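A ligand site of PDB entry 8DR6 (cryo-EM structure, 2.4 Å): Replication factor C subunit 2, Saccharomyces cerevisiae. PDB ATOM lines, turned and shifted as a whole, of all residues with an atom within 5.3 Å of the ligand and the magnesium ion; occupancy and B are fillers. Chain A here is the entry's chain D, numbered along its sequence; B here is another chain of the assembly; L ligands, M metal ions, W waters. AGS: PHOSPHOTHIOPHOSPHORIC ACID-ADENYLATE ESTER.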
ATOM      1  N   TRP A  27      26.214 -16.111   1.463  1.00  0.00           N
ATOM      2  CA  TRP A  27      26.176 -14.967   2.365  1.00  0.00           C
ATOM      3  C   TRP A  27      25.405 -15.270   3.643  1.00  0.00           C
ATOM      4  O   TRP A  27      25.702 -14.702   4.706  1.00  0.00           O
ATOM      5  CB  TRP A  27      25.570 -13.757   1.656  1.00  0.00           C
ATOM      6  CG  TRP A  27      26.436 -13.195   0.576  1.00  0.00           C
ATOM      7  CD1 TRP A  27      27.568 -13.753   0.046  1.00  0.00           C
ATOM      8  CD2 TRP A  27      26.251 -11.950  -0.109  1.00  0.00           C
ATOM      9  NE1 TRP A  27      28.096 -12.938  -0.916  1.00  0.00           N
ATOM     10  CE2 TRP A  27      27.305 -11.820  -1.043  1.00  0.00           C
ATOM     11  CE3 TRP A  27      25.299 -10.931  -0.033  1.00  0.00           C
ATOM     12  CZ2 TRP A  27      27.433 -10.719  -1.880  1.00  0.00           C
ATOM     13  CZ3 TRP A  27      25.427  -9.830  -0.870  1.00  0.00           C
ATOM     14  CH2 TRP A  27      26.488  -9.734  -1.782  1.00  0.00           C
ATOM     15  N   VAL A  28      24.407 -16.162   3.574  1.00  0.00           N
ATOM     16  CA  VAL A  28      23.656 -16.506   4.785  1.00  0.00           C
ATOM     17  C   VAL A  28      24.573 -17.154   5.822  1.00  0.00           C
ATOM     18  O   VAL A  28      24.518 -16.801   7.001  1.00  0.00           O
ATOM     19  CB  VAL A  28      22.465 -17.406   4.437  1.00  0.00           C
ATOM     20  CG1 VAL A  28      21.477 -16.673   3.551  1.00  0.00           C
ATOM     21  CG2 VAL A  28      22.924 -18.707   3.769  1.00  0.00           C
ATOM     22  N   GLU A  29      25.413 -18.099   5.403  1.00  0.00           N
ATOM     23  CA  GLU A  29      26.361 -18.741   6.299  1.00  0.00           C
ATOM     24  C   GLU A  29      27.570 -17.859   6.579  1.00  0.00           C
ATOM     25  O   GLU A  29      28.119 -17.894   7.688  1.00  0.00           O
ATOM     26  CB  GLU A  29      26.816 -20.079   5.724  1.00  0.00           C
ATOM     27  CG  GLU A  29      25.745 -21.167   5.728  1.00  0.00           C
ATOM     28  CD  GLU A  29      25.162 -21.425   7.110  1.00  0.00           C
ATOM     29  OE1 GLU A  29      25.689 -22.296   7.828  1.00  0.00           O
ATOM     30  OE2 GLU A  29      24.175 -20.742   7.479  1.00  0.00           O
ATOM     31  N   TYR A  31      27.787 -14.575   6.882  1.00  0.00           N
ATOM     32  CA  TYR A  31      27.503 -13.492   7.799  1.00  0.00           C
ATOM     33  C   TYR A  31      26.634 -13.940   8.975  1.00  0.00           C
ATOM     34  O   TYR A  31      25.929 -13.124   9.572  1.00  0.00           O
ATOM     35  CB  TYR A  31      26.820 -12.341   7.056  1.00  0.00           C
ATOM     36  CG  TYR A  31      27.750 -11.613   6.108  1.00  0.00           C
ATOM     37  CD1 TYR A  31      28.629 -10.644   6.584  1.00  0.00           C
ATOM     38  CD2 TYR A  31      27.759 -11.903   4.755  1.00  0.00           C
ATOM     39  CE1 TYR A  31      29.485  -9.975   5.721  1.00  0.00           C
ATOM     40  CE2 TYR A  31      28.605 -11.248   3.887  1.00  0.00           C
ATOM     41  CZ  TYR A  31      29.473 -10.282   4.375  1.00  0.00           C
ATOM     42  OH  TYR A  31      30.318  -9.630   3.520  1.00  0.00           O
ATOM     43  N   ARG A  32      26.685 -15.220   9.321  1.00  0.00           N
ATOM     44  CA  ARG A  32      25.977 -15.688  10.507  1.00  0.00           C
ATOM     45  C   ARG A  32      26.563 -15.019  11.748  1.00  0.00           C
ATOM     46  O   ARG A  32      27.785 -14.852  11.827  1.00  0.00           O
ATOM     47  CB  ARG A  32      26.089 -17.215  10.623  1.00  0.00           C
ATOM     48  CG  ARG A  32      25.291 -17.804  11.787  1.00  0.00           C
ATOM     49  CD  ARG A  32      25.415 -19.319  11.827  1.00  0.00           C
ATOM     50  NE  ARG A  32      24.618 -19.965  10.789  1.00  0.00           N
ATOM     51  CZ  ARG A  32      23.310 -20.198  10.879  1.00  0.00           C
ATOM     52  NH1 ARG A  32      22.614 -19.844  11.958  1.00  0.00           N
ATOM     53  NH2 ARG A  32      22.682 -20.795   9.871  1.00  0.00           N
ATOM     54  N   PRO A  33      25.741 -14.626  12.715  1.00  0.00           N
ATOM     55  CA  PRO A  33      26.292 -13.977  13.917  1.00  0.00           C
ATOM     56  C   PRO A  33      27.329 -14.847  14.598  1.00  0.00           C
ATOM     57  O   PRO A  33      27.143 -16.060  14.765  1.00  0.00           O
ATOM     58  CB  PRO A  33      25.055 -13.780  14.804  1.00  0.00           C
ATOM     59  CG  PRO A  33      23.919 -13.713  13.853  1.00  0.00           C
ATOM     60  CD  PRO A  33      24.272 -14.650  12.739  1.00  0.00           C
ATOM     61  N   GLU A  38      26.208  -9.483  17.730  1.00  0.00           N
ATOM     62  CA  GLU A  38      25.876  -9.381  16.315  1.00  0.00           C
ATOM     63  C   GLU A  38      24.400  -9.640  16.021  1.00  0.00           C
ATOM     64  O   GLU A  38      23.946  -9.360  14.907  1.00  0.00           O
ATOM     65  CB  GLU A  38      26.733 -10.356  15.493  1.00  0.00           C
ATOM     66  CG  GLU A  38      28.223 -10.226  15.749  1.00  0.00           C
ATOM     67  CD  GLU A  38      29.047 -10.415  14.495  1.00  0.00           C
ATOM     68  OE1 GLU A  38      29.166 -11.561  14.016  1.00  0.00           O
ATOM     69  OE2 GLU A  38      29.574  -9.410  13.971  1.00  0.00           O
ATOM     70  N   VAL A  39      23.651 -10.158  16.997  1.00  0.00           N
ATOM     71  CA  VAL A  39      22.213 -10.316  16.800  1.00  0.00           C
ATOM     72  C   VAL A  39      21.568  -8.937  16.724  1.00  0.00           C
ATOM     73  O   VAL A  39      21.876  -8.040  17.519  1.00  0.00           O
ATOM     74  CB  VAL A  39      21.598 -11.157  17.942  1.00  0.00           C
ATOM     75  CG1 VAL A  39      20.130 -11.441  17.665  1.00  0.00           C
ATOM     76  CG2 VAL A  39      22.381 -12.455  18.117  1.00  0.00           C
ATOM     77  N   THR A  40      20.678  -8.764  15.755  1.00  0.00           N
ATOM     78  CA  THR A  40      20.219  -7.425  15.364  1.00  0.00           C
ATOM     79  C   THR A  40      19.041  -6.940  16.215  1.00  0.00           C
ATOM     80  O   THR A  40      19.142  -5.922  16.907  1.00  0.00           O
ATOM     81  CB  THR A  40      19.866  -7.400  13.876  1.00  0.00           C
ATOM     82  OG1 THR A  40      20.929  -7.969  13.120  1.00  0.00           O
ATOM     83  CG2 THR A  40      19.612  -5.977  13.404  1.00  0.00           C
ATOM     84  N   ALA A  41      17.930  -7.667  16.172  1.00  0.00           N
ATOM     85  CA  ALA A  41      16.671  -7.193  16.736  1.00  0.00           C
ATOM     86  C   ALA A  41      16.042  -8.213  17.690  1.00  0.00           C
ATOM     87  O   ALA A  41      14.850  -8.493  17.601  1.00  0.00           O
ATOM     88  CB  ALA A  41      15.683  -6.846  15.612  1.00  0.00           C
ATOM     89  N   GLN A  42      16.835  -8.756  18.610  1.00  0.00           N
ATOM     90  CA  GLN A  42      16.335  -9.642  19.654  1.00  0.00           C
ATOM     91  C   GLN A  42      16.861  -9.209  21.019  1.00  0.00           C
ATOM     92  O   GLN A  42      17.221 -10.047  21.846  1.00  0.00           O
ATOM     93  CB  GLN A  42      16.719 -11.089  19.359  1.00  0.00           C
ATOM     94  CG  GLN A  42      16.414 -11.530  17.936  1.00  0.00           C
ATOM     95  CD  GLN A  42      14.934 -11.535  17.617  1.00  0.00           C
ATOM     96  OE1 GLN A  42      14.097 -11.231  18.471  1.00  0.00           O
ATOM     97  NE2 GLN A  42      14.592 -11.885  16.382  1.00  0.00           N
ATOM     98  N   GLY A  65       9.654 -18.742  17.319  1.00  0.00           N
ATOM     99  CA  GLY A  65       9.487 -17.621  16.430  1.00  0.00           C
ATOM    100  C   GLY A  65       9.418 -18.055  14.977  1.00  0.00           C
ATOM    101  O   GLY A  65       9.576 -19.239  14.656  1.00  0.00           O
ATOM    102  N   PRO A  66       9.202 -17.114  14.071  1.00  0.00           N
ATOM    103  CA  PRO A  66       9.089 -17.456  12.650  1.00  0.00           C
ATOM    104  C   PRO A  66      10.446 -17.755  12.042  1.00  0.00           C
ATOM    105  O   PRO A  66      11.480 -17.490  12.671  1.00  0.00           O
ATOM    106  CB  PRO A  66       8.460 -16.189  12.032  1.00  0.00           C
ATOM    107  CG  PRO A  66       8.865 -15.084  12.938  1.00  0.00           C
ATOM    108  CD  PRO A  66       9.027 -15.671  14.315  1.00  0.00           C
ATOM    109  N   PRO A  67      10.483 -18.299  10.834  1.00  0.00           N
ATOM    110  CA  PRO A  67      11.758 -18.683  10.230  1.00  0.00           C
ATOM    111  C   PRO A  67      12.685 -17.486  10.033  1.00  0.00           C
ATOM    112  O   PRO A  67      12.232 -16.355   9.804  1.00  0.00           O
ATOM    113  CB  PRO A  67      11.349 -19.300   8.887  1.00  0.00           C
ATOM    114  CG  PRO A  67       9.943 -19.738   9.088  1.00  0.00           C
ATOM    115  CD  PRO A  67       9.337 -18.704   9.991  1.00  0.00           C
ATOM    116  N   GLY A  68      13.984 -17.742  10.120  1.00  0.00           N
ATOM    117  CA  GLY A  68      14.973 -16.723   9.829  1.00  0.00           C
ATOM    118  C   GLY A  68      14.960 -15.536  10.768  1.00  0.00           C
ATOM    119  O   GLY A  68      15.003 -14.382  10.322  1.00  0.00           O
ATOM    120  N   THR A  69      14.892 -15.791  12.078  1.00  0.00           N
ATOM    121  CA  THR A  69      14.890 -14.735  13.074  1.00  0.00           C
ATOM    122  C   THR A  69      16.126 -14.741  13.966  1.00  0.00           C
ATOM    123  O   THR A  69      16.331 -13.775  14.705  1.00  0.00           O
ATOM    124  CB  THR A  69      13.641 -14.829  13.960  1.00  0.00           C
ATOM    125  OG1 THR A  69      13.473 -16.173  14.420  1.00  0.00           O
ATOM    126  CG2 THR A  69      12.401 -14.401  13.188  1.00  0.00           C
ATOM    127  N   GLY A  70      16.942 -15.787  13.923  1.00  0.00           N
ATOM    128  CA  GLY A  70      18.166 -15.847  14.682  1.00  0.00           C
ATOM    129  C   GLY A  70      18.141 -16.695  15.944  1.00  0.00           C
ATOM    130  O   GLY A  70      18.792 -16.315  16.923  1.00  0.00           O
ATOM    131  N   LYS A  71      17.414 -17.816  15.946  1.00  0.00           N
ATOM    132  CA  LYS A  71      17.369 -18.659  17.132  1.00  0.00           C
ATOM    133  C   LYS A  71      18.603 -19.556  17.210  1.00  0.00           C
ATOM    134  O   LYS A  71      19.305 -19.573  18.235  1.00  0.00           O
ATOM    135  CB  LYS A  71      16.090 -19.501  17.124  1.00  0.00           C
ATOM    136  CG  LYS A  71      14.816 -18.663  17.042  1.00  0.00           C
ATOM    137  CD  LYS A  71      13.563 -19.525  17.062  1.00  0.00           C
ATOM    138  CE  LYS A  71      13.415 -20.358  15.791  1.00  0.00           C
ATOM    139  NZ  LYS A  71      13.231 -19.521  14.577  1.00  0.00           N
ATOM    140  N   THR A  72      18.880 -20.304  16.147  1.00  0.00           N
ATOM    141  CA  THR A  72      20.058 -21.163  16.123  1.00  0.00           C
ATOM    142  C   THR A  72      21.328 -20.333  16.266  1.00  0.00           C
ATOM    143  O   THR A  72      22.250 -20.708  16.997  1.00  0.00           O
ATOM    144  CB  THR A  72      20.094 -21.986  14.837  1.00  0.00           C
ATOM    145  OG1 THR A  72      19.151 -23.064  14.936  1.00  0.00           O
ATOM    146  CG2 THR A  72      21.480 -22.547  14.579  1.00  0.00           C
ATOM    147  N   SER A  73      21.396 -19.202  15.568  1.00  0.00           N
ATOM    148  CA  SER A  73      22.556 -18.321  15.701  1.00  0.00           C
ATOM    149  C   SER A  73      22.709 -17.836  17.135  1.00  0.00           C
ATOM    150  O   SER A  73      23.825 -17.808  17.672  1.00  0.00           O
ATOM    151  CB  SER A  73      22.430 -17.139  14.745  1.00  0.00           C
ATOM    152  OG  SER A  73      22.458 -17.559  13.390  1.00  0.00           O
ATOM    153  N   ASP A 140      17.025 -28.822  18.739  1.00  0.00           N
ATOM    154  CA  ASP A 140      16.562 -27.980  17.648  1.00  0.00           C
ATOM    155  C   ASP A 140      15.383 -28.633  16.951  1.00  0.00           C
ATOM    156  O   ASP A 140      15.307 -29.864  16.849  1.00  0.00           O
ATOM    157  CB  ASP A 140      17.697 -27.735  16.644  1.00  0.00           C
ATOM    158  CG  ASP A 140      17.524 -26.434  15.880  1.00  0.00           C
ATOM    159  OD1 ASP A 140      16.501 -25.741  16.084  1.00  0.00           O
ATOM    160  OD2 ASP A 140      18.419 -26.094  15.080  1.00  0.00           O
ATOM    161  N   GLU A 141      14.449 -27.808  16.464  1.00  0.00           N
ATOM    162  CA  GLU A 141      13.233 -28.295  15.826  1.00  0.00           C
ATOM    163  C   GLU A 141      12.476 -29.247  16.757  1.00  0.00           C
ATOM    164  O   GLU A 141      12.012 -30.301  16.342  1.00  0.00           O
ATOM    165  CB  GLU A 141      13.540 -28.966  14.486  1.00  0.00           C
ATOM    166  CG  GLU A 141      13.997 -27.997  13.397  1.00  0.00           C
ATOM    167  CD  GLU A 141      15.432 -28.219  12.953  1.00  0.00           C
ATOM    168  OE1 GLU A 141      16.006 -29.279  13.261  1.00  0.00           O
ATOM    169  OE2 GLU A 141      15.988 -27.319  12.296  1.00  0.00           O
ATOM    170  N   ASN A 171       9.460 -23.590  15.778  1.00  0.00           N
ATOM    171  CA  ASN A 171       8.740 -22.579  15.008  1.00  0.00           C
ATOM    172  C   ASN A 171       7.274 -22.506  15.374  1.00  0.00           C
ATOM    173  O   ASN A 171       6.667 -21.438  15.232  1.00  0.00           O
ATOM    174  CB  ASN A 171       8.872 -22.864  13.504  1.00  0.00           C
ATOM    175  CG  ASN A 171      10.244 -22.540  12.967  1.00  0.00           C
ATOM    176  OD1 ASN A 171      10.977 -23.430  12.524  1.00  0.00           O
ATOM    177  ND2 ASN A 171      10.615 -21.267  12.990  1.00  0.00           N
ATOM    178  N   LEU A 192      11.780  -9.926  11.572  1.00  0.00           N
ATOM    179  CA  LEU A 192      12.776  -8.944  11.162  1.00  0.00           C
ATOM    180  C   LEU A 192      12.260  -8.200   9.935  1.00  0.00           C
ATOM    181  O   LEU A 192      12.168  -8.764   8.851  1.00  0.00           O
ATOM    182  CB  LEU A 192      14.116  -9.628  10.866  1.00  0.00           C
ATOM    183  CG  LEU A 192      14.701 -10.441  12.027  1.00  0.00           C
ATOM    184  CD1 LEU A 192      15.978 -11.138  11.601  1.00  0.00           C
ATOM    185  CD2 LEU A 192      14.960  -9.553  13.232  1.00  0.00           C
ATOM    186  N   ARG A 200      21.628  -4.300   9.642  1.00  0.00           N
ATOM    187  CA  ARG A 200      22.412  -5.496   9.320  1.00  0.00           C
ATOM    188  C   ARG A 200      22.525  -5.678   7.810  1.00  0.00           C
ATOM    189  O   ARG A 200      23.605  -5.996   7.304  1.00  0.00           O
ATOM    190  CB  ARG A 200      21.773  -6.718   9.972  1.00  0.00           C
ATOM    191  CG  ARG A 200      22.539  -8.017   9.769  1.00  0.00           C
ATOM    192  CD  ARG A 200      23.879  -8.001  10.498  1.00  0.00           C
ATOM    193  NE  ARG A 200      24.641  -9.218  10.256  1.00  0.00           N
ATOM    194  CZ  ARG A 200      25.849  -9.458  10.768  1.00  0.00           C
ATOM    195  NH1 ARG A 200      26.451  -8.581  11.556  1.00  0.00           N
ATOM    196  NH2 ARG A 200      26.456 -10.603  10.485  1.00  0.00           N
ATOM    197  N   LEU A 228      15.149 -12.681   7.489  1.00  0.00           N
ATOM    198  CA  LEU A 228      16.392 -12.025   7.098  1.00  0.00           C
ATOM    199  C   LEU A 228      17.241 -12.906   6.195  1.00  0.00           C
ATOM    200  O   LEU A 228      17.973 -12.383   5.344  1.00  0.00           O
ATOM    201  CB  LEU A 228      17.187 -11.628   8.345  1.00  0.00           C
ATOM    202  CG  LEU A 228      18.488 -10.866   8.122  1.00  0.00           C
ATOM    203  CD1 LEU A 228      18.304  -9.716   7.142  1.00  0.00           C
ATOM    204  CD2 LEU A 228      19.030 -10.343   9.445  1.00  0.00           C
ATOM    205  N   ARG A 229      17.156 -14.225   6.358  1.00  0.00           N
ATOM    206  CA  ARG A 229      17.901 -15.130   5.478  1.00  0.00           C
ATOM    207  C   ARG A 229      17.452 -14.965   4.033  1.00  0.00           C
ATOM    208  O   ARG A 229      18.281 -14.910   3.114  1.00  0.00           O
ATOM    209  CB  ARG A 229      17.702 -16.576   5.938  1.00  0.00           C
ATOM    210  CG  ARG A 229      18.593 -17.579   5.231  1.00  0.00           C
ATOM    211  CD  ARG A 229      18.032 -18.996   5.329  1.00  0.00           C
ATOM    212  NE  ARG A 229      18.307 -19.623   6.617  1.00  0.00           N
ATOM    213  CZ  ARG A 229      17.403 -19.868   7.558  1.00  0.00           C
ATOM    214  NH1 ARG A 229      16.126 -19.542   7.397  1.00  0.00           N
ATOM    215  NH2 ARG A 229      17.782 -20.459   8.687  1.00  0.00           N
ATOM    216  N   ILE A 232      18.866 -11.707   2.669  1.00  0.00           N
ATOM    217  CA  ILE A 232      20.294 -11.815   2.355  1.00  0.00           C
ATOM    218  C   ILE A 232      20.501 -12.597   1.067  1.00  0.00           C
ATOM    219  O   ILE A 232      21.331 -12.236   0.233  1.00  0.00           O
ATOM    220  CB  ILE A 232      21.048 -12.441   3.543  1.00  0.00           C
ATOM    221  CG1 ILE A 232      20.994 -11.519   4.755  1.00  0.00           C
ATOM    222  CG2 ILE A 232      22.497 -12.718   3.145  1.00  0.00           C
ATOM    223  CD1 ILE A 232      21.357 -12.191   6.059  1.00  0.00           C
ATOM    224  N   ARG B 155      16.592 -29.586   6.949  1.00  0.00           N
ATOM    225  CA  ARG B 155      16.828 -28.201   7.355  1.00  0.00           C
ATOM    226  C   ARG B 155      18.286 -27.987   7.768  1.00  0.00           C
ATOM    227  O   ARG B 155      19.009 -27.219   7.132  1.00  0.00           O
ATOM    228  CB  ARG B 155      15.881 -27.825   8.492  1.00  0.00           C
ATOM    229  CG  ARG B 155      14.453 -27.590   8.035  1.00  0.00           C
ATOM    230  CD  ARG B 155      13.499 -27.449   9.207  1.00  0.00           C
ATOM    231  NE  ARG B 155      13.860 -26.319  10.068  1.00  0.00           N
ATOM    232  CZ  ARG B 155      13.080 -25.843  11.026  1.00  0.00           C
ATOM    233  NH1 ARG B 155      11.887 -26.357  11.290  1.00  0.00           N
ATOM    234  NH2 ARG B 155      13.510 -24.810  11.754  1.00  0.00           N
ATOM    235  N   ARG B 156      18.725 -28.661   8.825  1.00  0.00           N
ATOM    236  CA  ARG B 156      20.054 -28.403   9.370  1.00  0.00           C
ATOM    237  C   ARG B 156      21.175 -28.957   8.494  1.00  0.00           C
ATOM    238  O   ARG B 156      22.307 -28.482   8.587  1.00  0.00           O
ATOM    239  CB  ARG B 156      20.172 -29.005  10.774  1.00  0.00           C
ATOM    240  CG  ARG B 156      19.437 -28.224  11.860  1.00  0.00           C
ATOM    241  CD  ARG B 156      20.024 -26.833  12.076  1.00  0.00           C
ATOM    242  NE  ARG B 156      21.401 -26.882  12.543  1.00  0.00           N
ATOM    243  CZ  ARG B 156      22.278 -25.891  12.405  1.00  0.00           C
ATOM    244  NH1 ARG B 156      21.947 -24.754  11.813  1.00  0.00           N
ATOM    245  NH2 ARG B 156      23.512 -26.041  12.878  1.00  0.00           N
ATOM    246  N   GLU B 159      22.647 -26.272   6.190  1.00  0.00           N
ATOM    247  CA  GLU B 159      23.378 -25.209   6.860  1.00  0.00           C
ATOM    248  C   GLU B 159      24.732 -25.656   7.399  1.00  0.00           C
ATOM    249  O   GLU B 159      25.745 -24.995   7.139  1.00  0.00           O
ATOM    250  CB  GLU B 159      22.542 -24.636   8.010  1.00  0.00           C
ATOM    251  CG  GLU B 159      21.148 -24.196   7.610  1.00  0.00           C
ATOM    252  CD  GLU B 159      20.405 -23.523   8.748  1.00  0.00           C
ATOM    253  OE1 GLU B 159      19.964 -24.225   9.678  1.00  0.00           O
ATOM    254  OE2 GLU B 159      20.259 -22.285   8.709  1.00  0.00           O
ATOM    255  N   PRO B 180      10.335 -23.285   6.134  1.00  0.00           N
ATOM    256  CA  PRO B 180      11.771 -23.296   6.479  1.00  0.00           C
ATOM    257  C   PRO B 180      12.659 -23.699   5.327  1.00  0.00           C
ATOM    258  O   PRO B 180      13.748 -23.140   5.163  1.00  0.00           O
ATOM    259  CB  PRO B 180      11.829 -24.304   7.639  1.00  0.00           C
ATOM    260  CG  PRO B 180      10.471 -24.279   8.237  1.00  0.00           C
ATOM    261  CD  PRO B 180       9.535 -24.078   7.091  1.00  0.00           C
ATOM    262  N   ARG B 184      15.627 -21.409   2.927  1.00  0.00           N
ATOM    263  CA  ARG B 184      17.019 -21.800   2.779  1.00  0.00           C
ATOM    264  C   ARG B 184      17.458 -21.944   1.325  1.00  0.00           C
ATOM    265  O   ARG B 184      18.591 -22.347   1.078  1.00  0.00           O
ATOM    266  CB  ARG B 184      17.286 -23.109   3.525  1.00  0.00           C
ATOM    267  CG  ARG B 184      17.181 -22.994   5.041  1.00  0.00           C
ATOM    268  CD  ARG B 184      17.248 -24.372   5.697  1.00  0.00           C
ATOM    269  NE  ARG B 184      17.509 -24.284   7.127  1.00  0.00           N
ATOM    270  CZ  ARG B 184      16.592 -23.992   8.047  1.00  0.00           C
ATOM    271  NH1 ARG B 184      15.338 -23.746   7.714  1.00  0.00           N
ATOM    272  NH2 ARG B 184      16.955 -23.943   9.328  1.00  0.00           N
HETATM  273  PG  AGS L   1      14.515 -21.461  11.561  1.00  0.00           P
HETATM  274  S1G AGS L   1      13.600 -22.022   9.939  1.00  0.00           S
HETATM  275  O2G AGS L   1      15.687 -22.443  11.858  1.00  0.00           O
HETATM  276  O3G AGS L   1      13.516 -21.479  12.753  1.00  0.00           O
HETATM  277  PB  AGS L   1      16.364 -19.540  12.161  1.00  0.00           P
HETATM  278  O1B AGS L   1      16.036 -18.459  13.108  1.00  0.00           O
HETATM  279  O2B AGS L   1      16.921 -20.786  12.861  1.00  0.00           O
HETATM  280  O3B AGS L   1      15.079 -20.014  11.376  1.00  0.00           O
HETATM  281  PA  AGS L   1      18.976 -18.883  11.593  1.00  0.00           P
HETATM  282  O1A AGS L   1      19.061 -18.452  13.003  1.00  0.00           O
HETATM  283  O2A AGS L   1      19.692 -20.209  11.317  1.00  0.00           O
HETATM  284  O3A AGS L   1      17.476 -19.078  11.127  1.00  0.00           O
HETATM  285  O5' AGS L   1      19.551 -17.729  10.679  1.00  0.00           O
HETATM  286  C5' AGS L   1      19.955 -17.977   9.320  1.00  0.00           C
HETATM  287  C4' AGS L   1      20.773 -16.818   8.826  1.00  0.00           C
HETATM  288  O4' AGS L   1      19.935 -15.647   8.743  1.00  0.00           O
HETATM  289  C3' AGS L   1      21.940 -16.414   9.731  1.00  0.00           C
HETATM  290  O3' AGS L   1      23.112 -17.146   9.406  1.00  0.00           O
HETATM  291  C2' AGS L   1      22.085 -14.922   9.437  1.00  0.00           C
HETATM  292  O2' AGS L   1      22.869 -14.678   8.279  1.00  0.00           O
HETATM  293  C1' AGS L   1      20.625 -14.499   9.214  1.00  0.00           C
HETATM  294  N9  AGS L   1      19.951 -14.024  10.423  1.00  0.00           N
HETATM  295  C8  AGS L   1      18.772 -14.492  10.944  1.00  0.00           C
HETATM  296  N7  AGS L   1      18.388 -13.878  12.038  1.00  0.00           N
HETATM  297  C5  AGS L   1      19.395 -12.943  12.258  1.00  0.00           C
HETATM  298  C6  AGS L   1      19.593 -11.984  13.259  1.00  0.00           C
HETATM  299  N6  AGS L   1      18.742 -11.780  14.277  1.00  0.00           N
HETATM  300  N1  AGS L   1      20.701 -11.207  13.188  1.00  0.00           N
HETATM  301  C2  AGS L   1      21.551 -11.398  12.173  1.00  0.00           C
HETATM  302  N3  AGS L   1      21.476 -12.279  11.166  1.00  0.00           N
HETATM  303  C4  AGS L   1      20.365 -13.027  11.265  1.00  0.00           C
HETATM  304 MG    MG M   1      17.422 -22.908  12.979  1.00  0.00          MG
HETATM  305  O   HOH W   1      18.818 -22.329  11.656  1.00  0.00           O
HETATM  306  O   HOH W   2      15.964 -23.039  14.340  1.00  0.00           O
HETATM  307  O   HOH W   3      17.336 -24.989  12.543  1.00  0.00           O
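The backbone NH (N) of Lys 71 lies within hydrogen-bond range of an oxygen (O1B) of the ligand (3.2 Å). O1B of the ligand lies within salt-bridge range of NZ of Lys 71 (3.3 Å). An oxygen (O3') of the ligand lies within hydrogen-bond range of the backbone carbonyl oxygen (O) of Val 28. An oxygen (O3B) of the ligand sits at hydrogen-bond distance from the backbone NH (N) of Gly 68 (2.8 Å). The guanidinium group (NH2) of Arg 229 is in salt-bridge range of an oxygen (O2A) of the ligand. ND2 of Asn 171 is in hydrogen-bond range of O3G of the ligand (2.9 Å). N of Gly 70 sits at hydrogen-bond distance from O1B of the ligand (2.9 Å). An oxygen (O2A) of the ligand is in salt-bridge range of the guanidinium group (NH1) of Arg 32, 3.0 Å away. The backbone NH of Thr 69 lies within hydrogen-bond range of an oxygen (O1B) of the ligand (3.1 Å). The backbone carbonyl oxygen of Thr 69 sits at hydrogen-bond distance from a nitrogen (N6) of the ligand. NH1 of Arg 184 of chain B lies close to S1G of the ligand, at 3.3 Å. A sulfur (S1G) of the ligand sits close to the guanidinium group (NH2) of Arg 155 of chain B. The side-chain hydroxyl of Thr 40 sits at hydrogen-bond distance from a nitrogen (N1) of the ligand (3.2 Å).
The backbone NH (N) of Leu 228 lies within hydrogen-bond range of the backbone carbonyl oxygen (O) of Gly 68 (3.3 Å). The side-chain amide oxygen (OD1) of Asn 171 lies within hydrogen-bond range of the guanidinium group (NH2) of Arg 155 of chain B (3.0 Å). OE2 of Glu 159 of chain B is in salt-bridge range of NH2 of Arg 32 (3.1 Å). NH2 of Arg 32 is in salt-bridge range of OE2 of Glu 29 (2.8 Å). The side-chain hydroxyl of Thr 69 sits at hydrogen-bond distance from the backbone carbonyl oxygen of Pro 66, at 3.0 Å. The backbone carbonyl oxygen of Arg 155 of chain B lies within hydrogen-bond range of the guanidinium group of Arg 184 of chain B, 3.3 Å away. O of Pro 180 of chain B lies within hydrogen-bond range of NH1 of Arg 184 of chain B, at 3.1 Å. NE of Arg 155 of chain B is in salt-bridge range of OE2 of Glu 141 (3.2 Å).
OE2 of Glu 159 of chain B sits close to O2A of the ligand (3.4 Å). Merely in contact with the ligand: Leu 228 (3.5 Å), Ser 73 (3.5 Å), Ile 232 (3.7 Å), Tyr 31 (3.7 Å), Leu 192 (3.7 Å), Val 39 (3.7 Å), Pro 67 (3.7 Å), Pro 180 of chain B (3.7 Å) and Pro 33 (3.7 Å). Hydrophobic or aromatic side chains within 4 Å of the ligand: Pro 33, Val 39, Pro 67, Leu 192, Leu 228, Ile 232 and Pro 180 of chain B. Of the 33 residues printed, 22 come within 4 Å of the ligand.
Asp 140 touches the magnesium ion (OD2 to MG, 3.9 Å). NH2 of Arg 184 of chain B touches the magnesium ion, at 3.8 Å. Within 4 Å of the magnesium ion: Thr 72, Asp 140 and Arg 184 of chain B.
The magnesium ion is bound by water W2. Water W1 is bound to the magnesium ion (2.0 Å). The magnesium ion is bound by O2G of the ligand, at 2.1 Å. Water W3 is bound to the magnesium ion, 2.1 Å away. An oxygen (O2B) of the ligand binds the magnesium ion, 2.2 Å away. The magnesium ion has five donor atoms within binding distance. Slightly farther from the magnesium ion lies the side-chain hydroxyl (OG1) of Thr 72 (2.6 Å).
Water W1 lies within hydrogen-bond range of OE1 of Glu 159 of chain B (3.0 Å), OG1 of Thr 72 (3.4 Å) and NH2 of Arg 184 of chain B (3.4 Å). Water W3 lies within hydrogen-bond range of the side-chain carboxylate (OE2) of Glu 141 (2.7 Å), the side-chain carboxylate (OD2) of Asp 140 (3.0 Å) and the guanidinium group (NH2) of Arg 184 of chain B (3.4 Å). Water W2 lies within hydrogen-bond range of the side-chain hydroxyl of Thr 72 (3.2 Å), the side-chain carboxylate of Asp 140 (3.3 Å) and an oxygen (O3G) of the ligand (3.3 Å).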
